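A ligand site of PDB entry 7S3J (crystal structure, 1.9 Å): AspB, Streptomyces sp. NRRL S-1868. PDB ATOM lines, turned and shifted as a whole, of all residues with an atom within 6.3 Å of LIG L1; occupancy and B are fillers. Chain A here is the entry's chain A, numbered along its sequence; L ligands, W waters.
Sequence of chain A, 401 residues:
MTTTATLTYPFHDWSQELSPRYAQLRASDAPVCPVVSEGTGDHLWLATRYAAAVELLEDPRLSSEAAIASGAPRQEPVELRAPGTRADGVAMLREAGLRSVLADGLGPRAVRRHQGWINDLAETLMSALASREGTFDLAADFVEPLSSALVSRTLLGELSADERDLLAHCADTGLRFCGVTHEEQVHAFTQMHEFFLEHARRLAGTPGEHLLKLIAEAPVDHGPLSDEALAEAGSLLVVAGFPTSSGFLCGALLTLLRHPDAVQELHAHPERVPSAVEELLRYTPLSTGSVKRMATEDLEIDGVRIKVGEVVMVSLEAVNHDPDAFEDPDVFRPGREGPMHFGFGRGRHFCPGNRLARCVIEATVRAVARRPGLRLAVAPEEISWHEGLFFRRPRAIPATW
Residues that only touch LIG L1: Gln 75 (3.5 Å), Glu 76 (3.3 Å), Thr 244 (3.7 Å), Leu 286 (3.97 Å), Gly 289 (3.9 Å), Ser 290 (3.7 Å), Val 291 (3.4 Å), Leu 316 (3.3 Å), Phe 390 (3.4 Å) and Phe 391 (3.7 Å).
12 residues have an atom within 4 Å of LIG L1: Gln 75, Glu 76, Thr 244, Leu 286, Ser 287, Gly 289, Ser 290, Val 291, Lys 292, Leu 316, Phe 390 and Phe 391.
The nearest printed residue that does not touch LIG L1 is Leu 80 (4.2 Å).
Water W2 lies within hydrogen-bond range of N3 of LIG L1 (2.7 Å), OE2 of Glu 317 (2.8 Å) and N of Ser 287 (3.3 Å).
Water W1 lies within hydrogen-bond range of an oxygen (O4) of LG2 L2 (2.5 Å), an oxygen (O1) of LIG L1 (2.8 Å) and the backbone NH of Lys 292 (2.9 Å).
Water W3 lies within hydrogen-bond range of the side-chain carboxylate (OE1) of Glu 317 (2.8 Å), the backbone carbonyl oxygen (O) of Gly 289 (2.8 Å) and the backbone NH (N) of Leu 316 (3.1 Å).
NZ of Lys 292 sits at hydrogen-bond distance from O1 of LIG L1.
OG of Ser 287 is in hydrogen-bond range of O2 of LIG L1 (3.2 Å).
NZ of Lys 292 lies within hydrogen-bond range of O1 of LG3 L3 (2.4 Å).
N1 of LG3 L3 lies within hydrogen-bond range of O2 of LG2 L2, at 2.7 Å.
The side-chain hydroxyl (OG) of Ser 287 is in hydrogen-bond range of the backbone NH (N) of Gly 289, at 2.9 Å.
The backbone NH of Ser 287 is in hydrogen-bond range of the side-chain carboxylate of Glu 317 (3.2 Å).
The backbone NH of Val 314 sits at hydrogen-bond distance from the backbone carbonyl oxygen of Val 291 (2.7 Å).
N of Thr 288 is in hydrogen-bond range of O of Phe 390 (2.8 Å).
The side-chain amide nitrogen of Gln 75 lies within hydrogen-bond range of the backbone carbonyl oxygen of Ser 290, at 2.9 Å.
The side-chain hydroxyl (OG1) of Thr 244 lies within hydrogen-bond range of the backbone carbonyl oxygen (O) of Ala 240 (2.6 Å).
OE2 of Glu 317 lies within hydrogen-bond range of N of Leu 286 (3.0 Å).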
ATOM      1  N   GLN A  75       7.960  -6.655  -3.534  1.00  0.00           N
ATOM      2  CA  GLN A  75       8.164  -5.232  -3.355  1.00  0.00           C
ATOM      3  C   GLN A  75       7.313  -4.373  -4.290  1.00  0.00           C
ATOM      4  O   GLN A  75       6.993  -3.237  -3.940  1.00  0.00           O
ATOM      5  CB  GLN A  75       9.659  -4.912  -3.537  1.00  0.00           C
ATOM      6  CG  GLN A  75      10.152  -4.985  -4.967  1.00  0.00           C
ATOM      7  CD  GLN A  75      11.672  -5.037  -5.024  1.00  0.00           C
ATOM      8  OE1 GLN A  75      12.341  -4.012  -4.885  1.00  0.00           O
ATOM      9  NE2 GLN A  75      12.229  -6.236  -5.201  1.00  0.00           N
ATOM     10  N   GLU A  76       6.882  -4.910  -5.487  1.00  0.00           N
ATOM     11  CA  GLU A  76       6.259  -4.030  -6.477  1.00  0.00           C
ATOM     12  C   GLU A  76       4.734  -3.957  -6.290  1.00  0.00           C
ATOM     13  O   GLU A  76       4.111  -4.901  -5.794  1.00  0.00           O
ATOM     14  CB  GLU A  76       6.603  -4.509  -7.884  1.00  0.00           C
ATOM     15  CG  GLU A  76       6.168  -5.933  -8.218  1.00  0.00           C
ATOM     16  CD  GLU A  76       7.167  -6.993  -7.772  1.00  0.00           C
ATOM     17  OE1 GLU A  76       7.990  -6.699  -6.883  1.00  0.00           O
ATOM     18  OE2 GLU A  76       7.138  -8.116  -8.310  1.00  0.00           O
ATOM     19  N   LEU A  80       4.366  -7.663 -12.645  1.00  0.00           N
ATOM     20  CA  LEU A  80       5.079  -7.173 -13.839  1.00  0.00           C
ATOM     21  C   LEU A  80       4.790  -8.105 -15.017  1.00  0.00           C
ATOM     22  O   LEU A  80       5.646  -8.814 -15.539  1.00  0.00           O
ATOM     23  CB  LEU A  80       6.576  -7.078 -13.565  1.00  0.00           C
ATOM     24  CG  LEU A  80       6.861  -6.429 -12.212  1.00  0.00           C
ATOM     25  CD1 LEU A  80       8.339  -6.477 -11.874  1.00  0.00           C
ATOM     26  CD2 LEU A  80       6.321  -5.026 -12.145  1.00  0.00           C
ATOM     27  N   PHE A 177       7.039   2.055  -8.604  1.00  0.00           N
ATOM     28  CA  PHE A 177       6.567   1.758  -7.277  1.00  0.00           C
ATOM     29  C   PHE A 177       5.340   2.609  -6.954  1.00  0.00           C
ATOM     30  O   PHE A 177       4.495   2.194  -6.213  1.00  0.00           O
ATOM     31  CB  PHE A 177       7.652   2.145  -6.292  1.00  0.00           C
ATOM     32  CG  PHE A 177       8.680   1.099  -6.076  1.00  0.00           C
ATOM     33  CD1 PHE A 177       8.335  -0.110  -5.509  1.00  0.00           C
ATOM     34  CD2 PHE A 177       9.997   1.320  -6.418  1.00  0.00           C
ATOM     35  CE1 PHE A 177       9.277  -1.087  -5.287  1.00  0.00           C
ATOM     36  CE2 PHE A 177      10.954   0.350  -6.211  1.00  0.00           C
ATOM     37  CZ  PHE A 177      10.584  -0.859  -5.642  1.00  0.00           C
ATOM     38  N   ALA A 240      13.898  -5.584 -19.813  1.00  0.00           N
ATOM     39  CA  ALA A 240      15.235  -5.818 -19.282  1.00  0.00           C
ATOM     40  C   ALA A 240      16.249  -4.821 -19.810  1.00  0.00           C
ATOM     41  O   ALA A 240      17.218  -4.509 -19.104  1.00  0.00           O
ATOM     42  CB  ALA A 240      15.699  -7.245 -19.593  1.00  0.00           C
ATOM     43  N   THR A 244      16.680   0.201 -18.087  1.00  0.00           N
ATOM     44  CA  THR A 244      17.956  -0.023 -17.422  1.00  0.00           C
ATOM     45  C   THR A 244      19.084   0.720 -18.147  1.00  0.00           C
ATOM     46  O   THR A 244      19.846   1.472 -17.536  1.00  0.00           O
ATOM     47  CB  THR A 244      18.229  -1.523 -17.407  1.00  0.00           C
ATOM     48  OG1 THR A 244      17.982  -2.018 -18.731  1.00  0.00           O
ATOM     49  CG2 THR A 244      17.257  -2.230 -16.444  1.00  0.00           C
ATOM     50  N   LEU A 286      21.375   2.681  -9.710  1.00  0.00           N
ATOM     51  CA  LEU A 286      20.340   2.528 -10.720  1.00  0.00           C
ATOM     52  C   LEU A 286      18.969   2.181 -10.118  1.00  0.00           C
ATOM     53  O   LEU A 286      18.042   2.965 -10.232  1.00  0.00           O
ATOM     54  CB  LEU A 286      20.776   1.474 -11.723  1.00  0.00           C
ATOM     55  CG  LEU A 286      19.761   1.228 -12.834  1.00  0.00           C
ATOM     56  CD1 LEU A 286      19.416   2.578 -13.599  1.00  0.00           C
ATOM     57  CD2 LEU A 286      20.262   0.128 -13.761  1.00  0.00           C
ATOM     58  N   SER A 287      18.833   1.058  -9.458  1.00  0.00           N
ATOM     59  CA  SER A 287      17.500   0.597  -9.080  1.00  0.00           C
ATOM     60  C   SER A 287      17.142   1.155  -7.724  1.00  0.00           C
ATOM     61  O   SER A 287      17.945   1.117  -6.797  1.00  0.00           O
ATOM     62  CB  SER A 287      17.424  -0.925  -9.070  1.00  0.00           C
ATOM     63  OG  SER A 287      16.302  -1.361  -8.354  1.00  0.00           O
ATOM     64  N   THR A 288      15.930   1.725  -7.641  1.00  0.00           N
ATOM     65  CA  THR A 288      15.320   2.115  -6.372  1.00  0.00           C
ATOM     66  C   THR A 288      14.777   0.915  -5.580  1.00  0.00           C
ATOM     67  O   THR A 288      14.335   1.117  -4.452  1.00  0.00           O
ATOM     68  CB  THR A 288      14.192   3.110  -6.611  1.00  0.00           C
ATOM     69  OG1 THR A 288      13.213   2.458  -7.424  1.00  0.00           O
ATOM     70  CG2 THR A 288      14.711   4.335  -7.336  1.00  0.00           C
ATOM     71  N   GLY A 289      14.752  -0.280  -6.166  1.00  0.00           N
ATOM     72  CA  GLY A 289      14.372  -1.491  -5.489  1.00  0.00           C
ATOM     73  C   GLY A 289      15.551  -2.427  -5.272  1.00  0.00           C
ATOM     74  O   GLY A 289      16.719  -2.014  -5.261  1.00  0.00           O
ATOM     75  N   SER A 290      15.250  -3.720  -5.113  1.00  0.00           N
ATOM     76  CA  SER A 290      16.280  -4.724  -4.830  1.00  0.00           C
ATOM     77  C   SER A 290      16.061  -5.947  -5.705  1.00  0.00           C
ATOM     78  O   SER A 290      14.946  -6.216  -6.161  1.00  0.00           O
ATOM     79  CB  SER A 290      16.281  -5.164  -3.356  1.00  0.00           C
ATOM     80  OG  SER A 290      16.519  -4.093  -2.464  1.00  0.00           O
ATOM     81  N   VAL A 291      17.148  -6.672  -5.986  1.00  0.00           N
ATOM     82  CA  VAL A 291      16.993  -8.027  -6.520  1.00  0.00           C
ATOM     83  C   VAL A 291      16.434  -8.911  -5.415  1.00  0.00           C
ATOM     84  O   VAL A 291      16.603  -8.622  -4.224  1.00  0.00           O
ATOM     85  CB  VAL A 291      18.331  -8.574  -7.062  1.00  0.00           C
ATOM     86  CG1 VAL A 291      18.984  -7.547  -7.953  1.00  0.00           C
ATOM     87  CG2 VAL A 291      19.249  -8.961  -5.918  1.00  0.00           C
ATOM     88  N   LYS A 292      15.727  -9.962  -5.779  1.00  0.00           N
ATOM     89  CA  LYS A 292      14.953 -10.660  -4.770  1.00  0.00           C
ATOM     90  C   LYS A 292      14.851 -12.138  -5.089  1.00  0.00           C
ATOM     91  O   LYS A 292      14.819 -12.533  -6.264  1.00  0.00           O
ATOM     92  CB  LYS A 292      13.538 -10.033  -4.579  1.00  0.00           C
ATOM     93  CG  LYS A 292      12.469 -10.483  -5.570  1.00  0.00           C
ATOM     94  CD  LYS A 292      12.713  -9.887  -6.956  1.00  0.00           C
ATOM     95  CE  LYS A 292      11.523 -10.078  -7.820  1.00  0.00           C
ATOM     96  NZ  LYS A 292      11.875 -10.121  -9.263  1.00  0.00           N
ATOM     97  N   VAL A 314      18.090  -8.110  -2.023  1.00  0.00           N
ATOM     98  CA  VAL A 314      19.443  -7.559  -1.913  1.00  0.00           C
ATOM     99  C   VAL A 314      19.489  -6.286  -2.754  1.00  0.00           C
ATOM    100  O   VAL A 314      19.283  -6.342  -3.970  1.00  0.00           O
ATOM    101  CB  VAL A 314      20.517  -8.543  -2.401  1.00  0.00           C
ATOM    102  CG1 VAL A 314      21.835  -7.821  -2.526  1.00  0.00           C
ATOM    103  CG2 VAL A 314      20.616  -9.772  -1.449  1.00  0.00           C
ATOM    104  N   LEU A 316      21.511  -3.821  -4.662  1.00  0.00           N
ATOM    105  CA  LEU A 316      22.826  -3.669  -5.293  1.00  0.00           C
ATOM    106  C   LEU A 316      23.467  -2.321  -4.953  1.00  0.00           C
ATOM    107  O   LEU A 316      24.698  -2.228  -4.811  1.00  0.00           O
ATOM    108  CB  LEU A 316      22.693  -3.811  -6.791  1.00  0.00           C
ATOM    109  CG  LEU A 316      21.892  -5.055  -7.130  1.00  0.00           C
ATOM    110  CD1 LEU A 316      21.659  -5.066  -8.604  1.00  0.00           C
ATOM    111  CD2 LEU A 316      22.670  -6.305  -6.690  1.00  0.00           C
ATOM    112  N   GLU A 317      22.652  -1.269  -4.819  1.00  0.00           N
ATOM    113  CA  GLU A 317      23.176   0.050  -4.464  1.00  0.00           C
ATOM    114  C   GLU A 317      23.847   0.037  -3.096  1.00  0.00           C
ATOM    115  O   GLU A 317      24.974   0.522  -2.941  1.00  0.00           O
ATOM    116  CB  GLU A 317      22.040   1.095  -4.478  1.00  0.00           C
ATOM    117  CG  GLU A 317      21.687   1.549  -5.897  1.00  0.00           C
ATOM    118  CD  GLU A 317      21.191   0.401  -6.742  1.00  0.00           C
ATOM    119  OE1 GLU A 317      20.466  -0.454  -6.189  1.00  0.00           O
ATOM    120  OE2 GLU A 317      21.558   0.330  -7.933  1.00  0.00           O
ATOM    121  N   GLY A 343      26.876  -4.528  -9.988  1.00  0.00           N
ATOM    122  CA  GLY A 343      26.089  -3.722 -10.896  1.00  0.00           C
ATOM    123  C   GLY A 343      25.255  -4.520 -11.881  1.00  0.00           C
ATOM    124  O   GLY A 343      24.193  -4.039 -12.315  1.00  0.00           O
ATOM    125  N   PHE A 390      11.344   2.379 -11.049  1.00  0.00           N
ATOM    126  CA  PHE A 390      12.239   1.332 -10.543  1.00  0.00           C
ATOM    127  C   PHE A 390      13.692   1.691 -10.867  1.00  0.00           C
ATOM    128  O   PHE A 390      14.604   1.498 -10.052  1.00  0.00           O
ATOM    129  CB  PHE A 390      11.891  -0.016 -11.166  1.00  0.00           C
ATOM    130  CG  PHE A 390      10.599  -0.635 -10.666  1.00  0.00           C
ATOM    131  CD1 PHE A 390       9.997  -0.191  -9.516  1.00  0.00           C
ATOM    132  CD2 PHE A 390      10.027  -1.695 -11.357  1.00  0.00           C
ATOM    133  CE1 PHE A 390       8.823  -0.772  -9.068  1.00  0.00           C
ATOM    134  CE2 PHE A 390       8.862  -2.274 -10.931  1.00  0.00           C
ATOM    135  CZ  PHE A 390       8.245  -1.819  -9.778  1.00  0.00           C
ATOM    136  N   PHE A 391      13.909   2.228 -12.063  1.00  0.00           N
ATOM    137  CA  PHE A 391      15.241   2.542 -12.585  1.00  0.00           C
ATOM    138  C   PHE A 391      15.375   4.066 -12.636  1.00  0.00           C
ATOM    139  O   PHE A 391      14.816   4.719 -13.525  1.00  0.00           O
ATOM    140  CB  PHE A 391      15.408   1.833 -13.926  1.00  0.00           C
ATOM    141  CG  PHE A 391      15.247   0.328 -13.814  1.00  0.00           C
ATOM    142  CD1 PHE A 391      16.021  -0.408 -12.907  1.00  0.00           C
ATOM    143  CD2 PHE A 391      14.301  -0.347 -14.545  1.00  0.00           C
ATOM    144  CE1 PHE A 391      15.860  -1.782 -12.752  1.00  0.00           C
ATOM    145  CE2 PHE A 391      14.146  -1.726 -14.405  1.00  0.00           C
ATOM    146  CZ  PHE A 391      14.932  -2.444 -13.505  1.00  0.00           C
HETATM  147  C1  LIG L   1      13.646  -6.386  -9.574  1.00  0.00           C
HETATM  148  N1  LIG L   1      14.670  -4.166  -9.670  1.00  0.00           N
HETATM  149  O1  LIG L   1      13.828  -7.579  -9.374  1.00  0.00           O
HETATM  150  C2  LIG L   1      14.790  -5.559 -10.075  1.00  0.00           C
HETATM  151  C3  LIG L   1      16.144  -6.211  -9.678  1.00  0.00           C
HETATM  152  C4  LIG L   1      17.256  -5.249 -10.033  1.00  0.00           C
HETATM  153  O2  LIG L   1      13.361  -2.401  -9.175  1.00  0.00           O
HETATM  154  C5  LIG L   1      10.374  -5.104  -8.502  1.00  0.00           C
HETATM  155  C6  LIG L   1      11.197  -3.885  -8.871  1.00  0.00           C
HETATM  156  C7  LIG L   1      11.276  -6.330  -8.720  1.00  0.00           C
HETATM  157  C8  LIG L   1      13.487  -3.564  -9.544  1.00  0.00           C
HETATM  158  C9  LIG L   1      12.263  -4.371  -9.818  1.00  0.00           C
HETATM  159  N2  LIG L   1      12.469  -5.771  -9.377  1.00  0.00           N
HETATM  160  C10 LIG L   1      18.035  -4.508  -9.154  1.00  0.00           C
HETATM  161  C11 LIG L   1      17.675  -4.897 -11.308  1.00  0.00           C
HETATM  162  N3  LIG L   1      18.896  -3.740  -9.888  1.00  0.00           N
HETATM  163  C12 LIG L   1      18.691  -3.969 -11.200  1.00  0.00           C
HETATM  164  C13 LIG L   1      17.212  -5.334 -12.531  1.00  0.00           C
HETATM  165  C14 LIG L   1      18.828  -3.906 -13.592  1.00  0.00           C
HETATM  166  C15 LIG L   1      19.280  -3.452 -12.360  1.00  0.00           C
HETATM  167  C16 LIG L   1      17.811  -4.841 -13.679  1.00  0.00           C
HETATM  168  C1  LG2 L   2      19.196  -9.215 -15.278  1.00  0.00           C
HETATM  169  C2  LG2 L   2      18.907  -8.239 -20.014  1.00  0.00           C
HETATM  170  C3  LG2 L   2      21.083  -4.053 -19.230  1.00  0.00           C
HETATM  171  C4  LG2 L   2      21.660  -5.102 -14.547  1.00  0.00           C
HETATM  172  C5  LG2 L   2      18.841  -9.269 -16.608  1.00  0.00           C
HETATM  173  C6  LG2 L   2      17.952 -10.253 -17.215  1.00  0.00           C
HETATM  174  C7  LG2 L   2      17.897  -9.973 -18.530  1.00  0.00           C
HETATM  175  C8  LG2 L   2      18.718  -8.814 -18.781  1.00  0.00           C
HETATM  176  C9  LG2 L   2      17.096 -10.682 -19.647  1.00  0.00           C
HETATM  177  C10 LG2 L   2      17.217 -11.420 -16.474  1.00  0.00           C
HETATM  178  C11 LG2 L   2      18.213 -12.434 -15.933  1.00  0.00           C
HETATM  179  C12 LG2 L   2      17.538 -13.497 -15.098  1.00  0.00           C
HETATM  180  O1  LG2 L   2      18.122 -14.611 -14.988  1.00  0.00           O
HETATM  181  O2  LG2 L   2      16.414 -13.256 -14.567  1.00  0.00           O
HETATM  182  C13 LG2 L   2      19.528  -7.042 -20.216  1.00  0.00           C
HETATM  183  C14 LG2 L   2      19.744  -6.434 -21.506  1.00  0.00           C
HETATM  184  C15 LG2 L   2      20.351  -5.253 -21.274  1.00  0.00           C
HETATM  185  C16 LG2 L   2      20.534  -5.129 -19.853  1.00  0.00           C
HETATM  186  C17 LG2 L   2      19.294  -7.132 -22.811  1.00  0.00           C
HETATM  187  C18 LG2 L   2      20.868  -4.174 -22.256  1.00  0.00           C
HETATM  188  C19 LG2 L   2      21.024  -4.399 -23.558  1.00  0.00           C
HETATM  189  C20 LG2 L   2      21.381  -3.975 -17.908  1.00  0.00           C
HETATM  190  C21 LG2 L   2      22.066  -2.839 -17.323  1.00  0.00           C
HETATM  191  C22 LG2 L   2      22.224  -3.130 -16.011  1.00  0.00           C
HETATM  192  C23 LG2 L   2      21.661  -4.447 -15.758  1.00  0.00           C
HETATM  193  C24 LG2 L   2      22.472  -1.569 -18.119  1.00  0.00           C
HETATM  194  C25 LG2 L   2      22.897  -2.288 -14.895  1.00  0.00           C
HETATM  195  C26 LG2 L   2      23.494  -1.118 -15.132  1.00  0.00           C
HETATM  196  C27 LG2 L   2      21.043  -6.311 -14.339  1.00  0.00           C
HETATM  197  C28 LG2 L   2      20.915  -6.980 -13.075  1.00  0.00           C
HETATM  198  C29 LG2 L   2      20.243  -8.107 -13.248  1.00  0.00           C
HETATM  199  C30 LG2 L   2      19.893  -8.208 -14.660  1.00  0.00           C
HETATM  200  C31 LG2 L   2      21.481  -6.416 -11.761  1.00  0.00           C
HETATM  201  C32 LG2 L   2      19.957  -9.150 -12.121  1.00  0.00           C
HETATM  202  C33 LG2 L   2      18.494  -9.450 -11.807  1.00  0.00           C
HETATM  203  C34 LG2 L   2      18.425 -10.360 -10.584  1.00  0.00           C
HETATM  204  O3  LG2 L   2      19.496 -10.803 -10.099  1.00  0.00           O
HETATM  205  O4  LG2 L   2      17.308 -10.661 -10.074  1.00  0.00           O
HETATM  206  N1  LG2 L   2      19.283  -8.397 -17.611  1.00  0.00           N
HETATM  207  N2  LG2 L   2      20.014  -6.215 -19.219  1.00  0.00           N
HETATM  208  N3  LG2 L   2      21.141  -4.939 -16.930  1.00  0.00           N
HETATM  209  N4  LG2 L   2      20.401  -7.088 -15.297  1.00  0.00           N
HETATM  210 FE1  LG2 L   2      20.400  -6.761 -17.354  1.00  0.00          FE
HETATM  211  C1  LG3 L   3      12.711 -10.267 -12.765  1.00  0.00           C
HETATM  212  N1  LG3 L   3      14.499 -11.332 -14.184  1.00  0.00           N
HETATM  213  O1  LG3 L   3      12.336  -9.913 -11.655  1.00  0.00           O
HETATM  214  C2  LG3 L   3      14.161 -10.659 -12.930  1.00  0.00           C
HETATM  215  C3  LG3 L   3      15.035  -9.424 -12.732  1.00  0.00           C
HETATM  216  C4  LG3 L   3      14.896  -8.349 -13.811  1.00  0.00           C
HETATM  217  O2  LG3 L   3      13.950 -12.273 -16.136  1.00  0.00           O
HETATM  218  C5  LG3 L   3      10.876  -8.967 -15.424  1.00  0.00           C
HETATM  219  C6  LG3 L   3      12.001  -9.779 -16.062  1.00  0.00           C
HETATM  220  C7  LG3 L   3      10.645  -9.546 -14.030  1.00  0.00           C
HETATM  221  C8  LG3 L   3      13.639 -11.557 -15.173  1.00  0.00           C
HETATM  222  C9  LG3 L   3      12.250 -10.940 -15.091  1.00  0.00           C
HETATM  223  N2  LG3 L   3      11.903 -10.261 -13.836  1.00  0.00           N
HETATM  224  C10 LG3 L   3      15.756  -8.161 -14.889  1.00  0.00           C
HETATM  225  C11 LG3 L   3      13.940  -7.328 -13.915  1.00  0.00           C
HETATM  226  N3  LG3 L   3      15.328  -7.090 -15.628  1.00  0.00           N
HETATM  227  C12 LG3 L   3      14.235  -6.568 -15.047  1.00  0.00           C
HETATM  228  C13 LG3 L   3      12.841  -7.018 -13.097  1.00  0.00           C
HETATM  229  C14 LG3 L   3      12.303  -5.177 -14.561  1.00  0.00           C
HETATM  230  C15 LG3 L   3      13.408  -5.482 -15.358  1.00  0.00           C
HETATM  231  C16 LG3 L   3      12.029  -5.943 -13.424  1.00  0.00           C
HETATM  232  O   HOH W   1      15.424  -9.813  -8.680  1.00  0.00           O
HETATM  233  O   HOH W   2      20.691  -1.692  -9.689  1.00  0.00           O
HETATM  234  O   HOH W   3      19.148  -2.891  -6.386  1.00  0.00           O
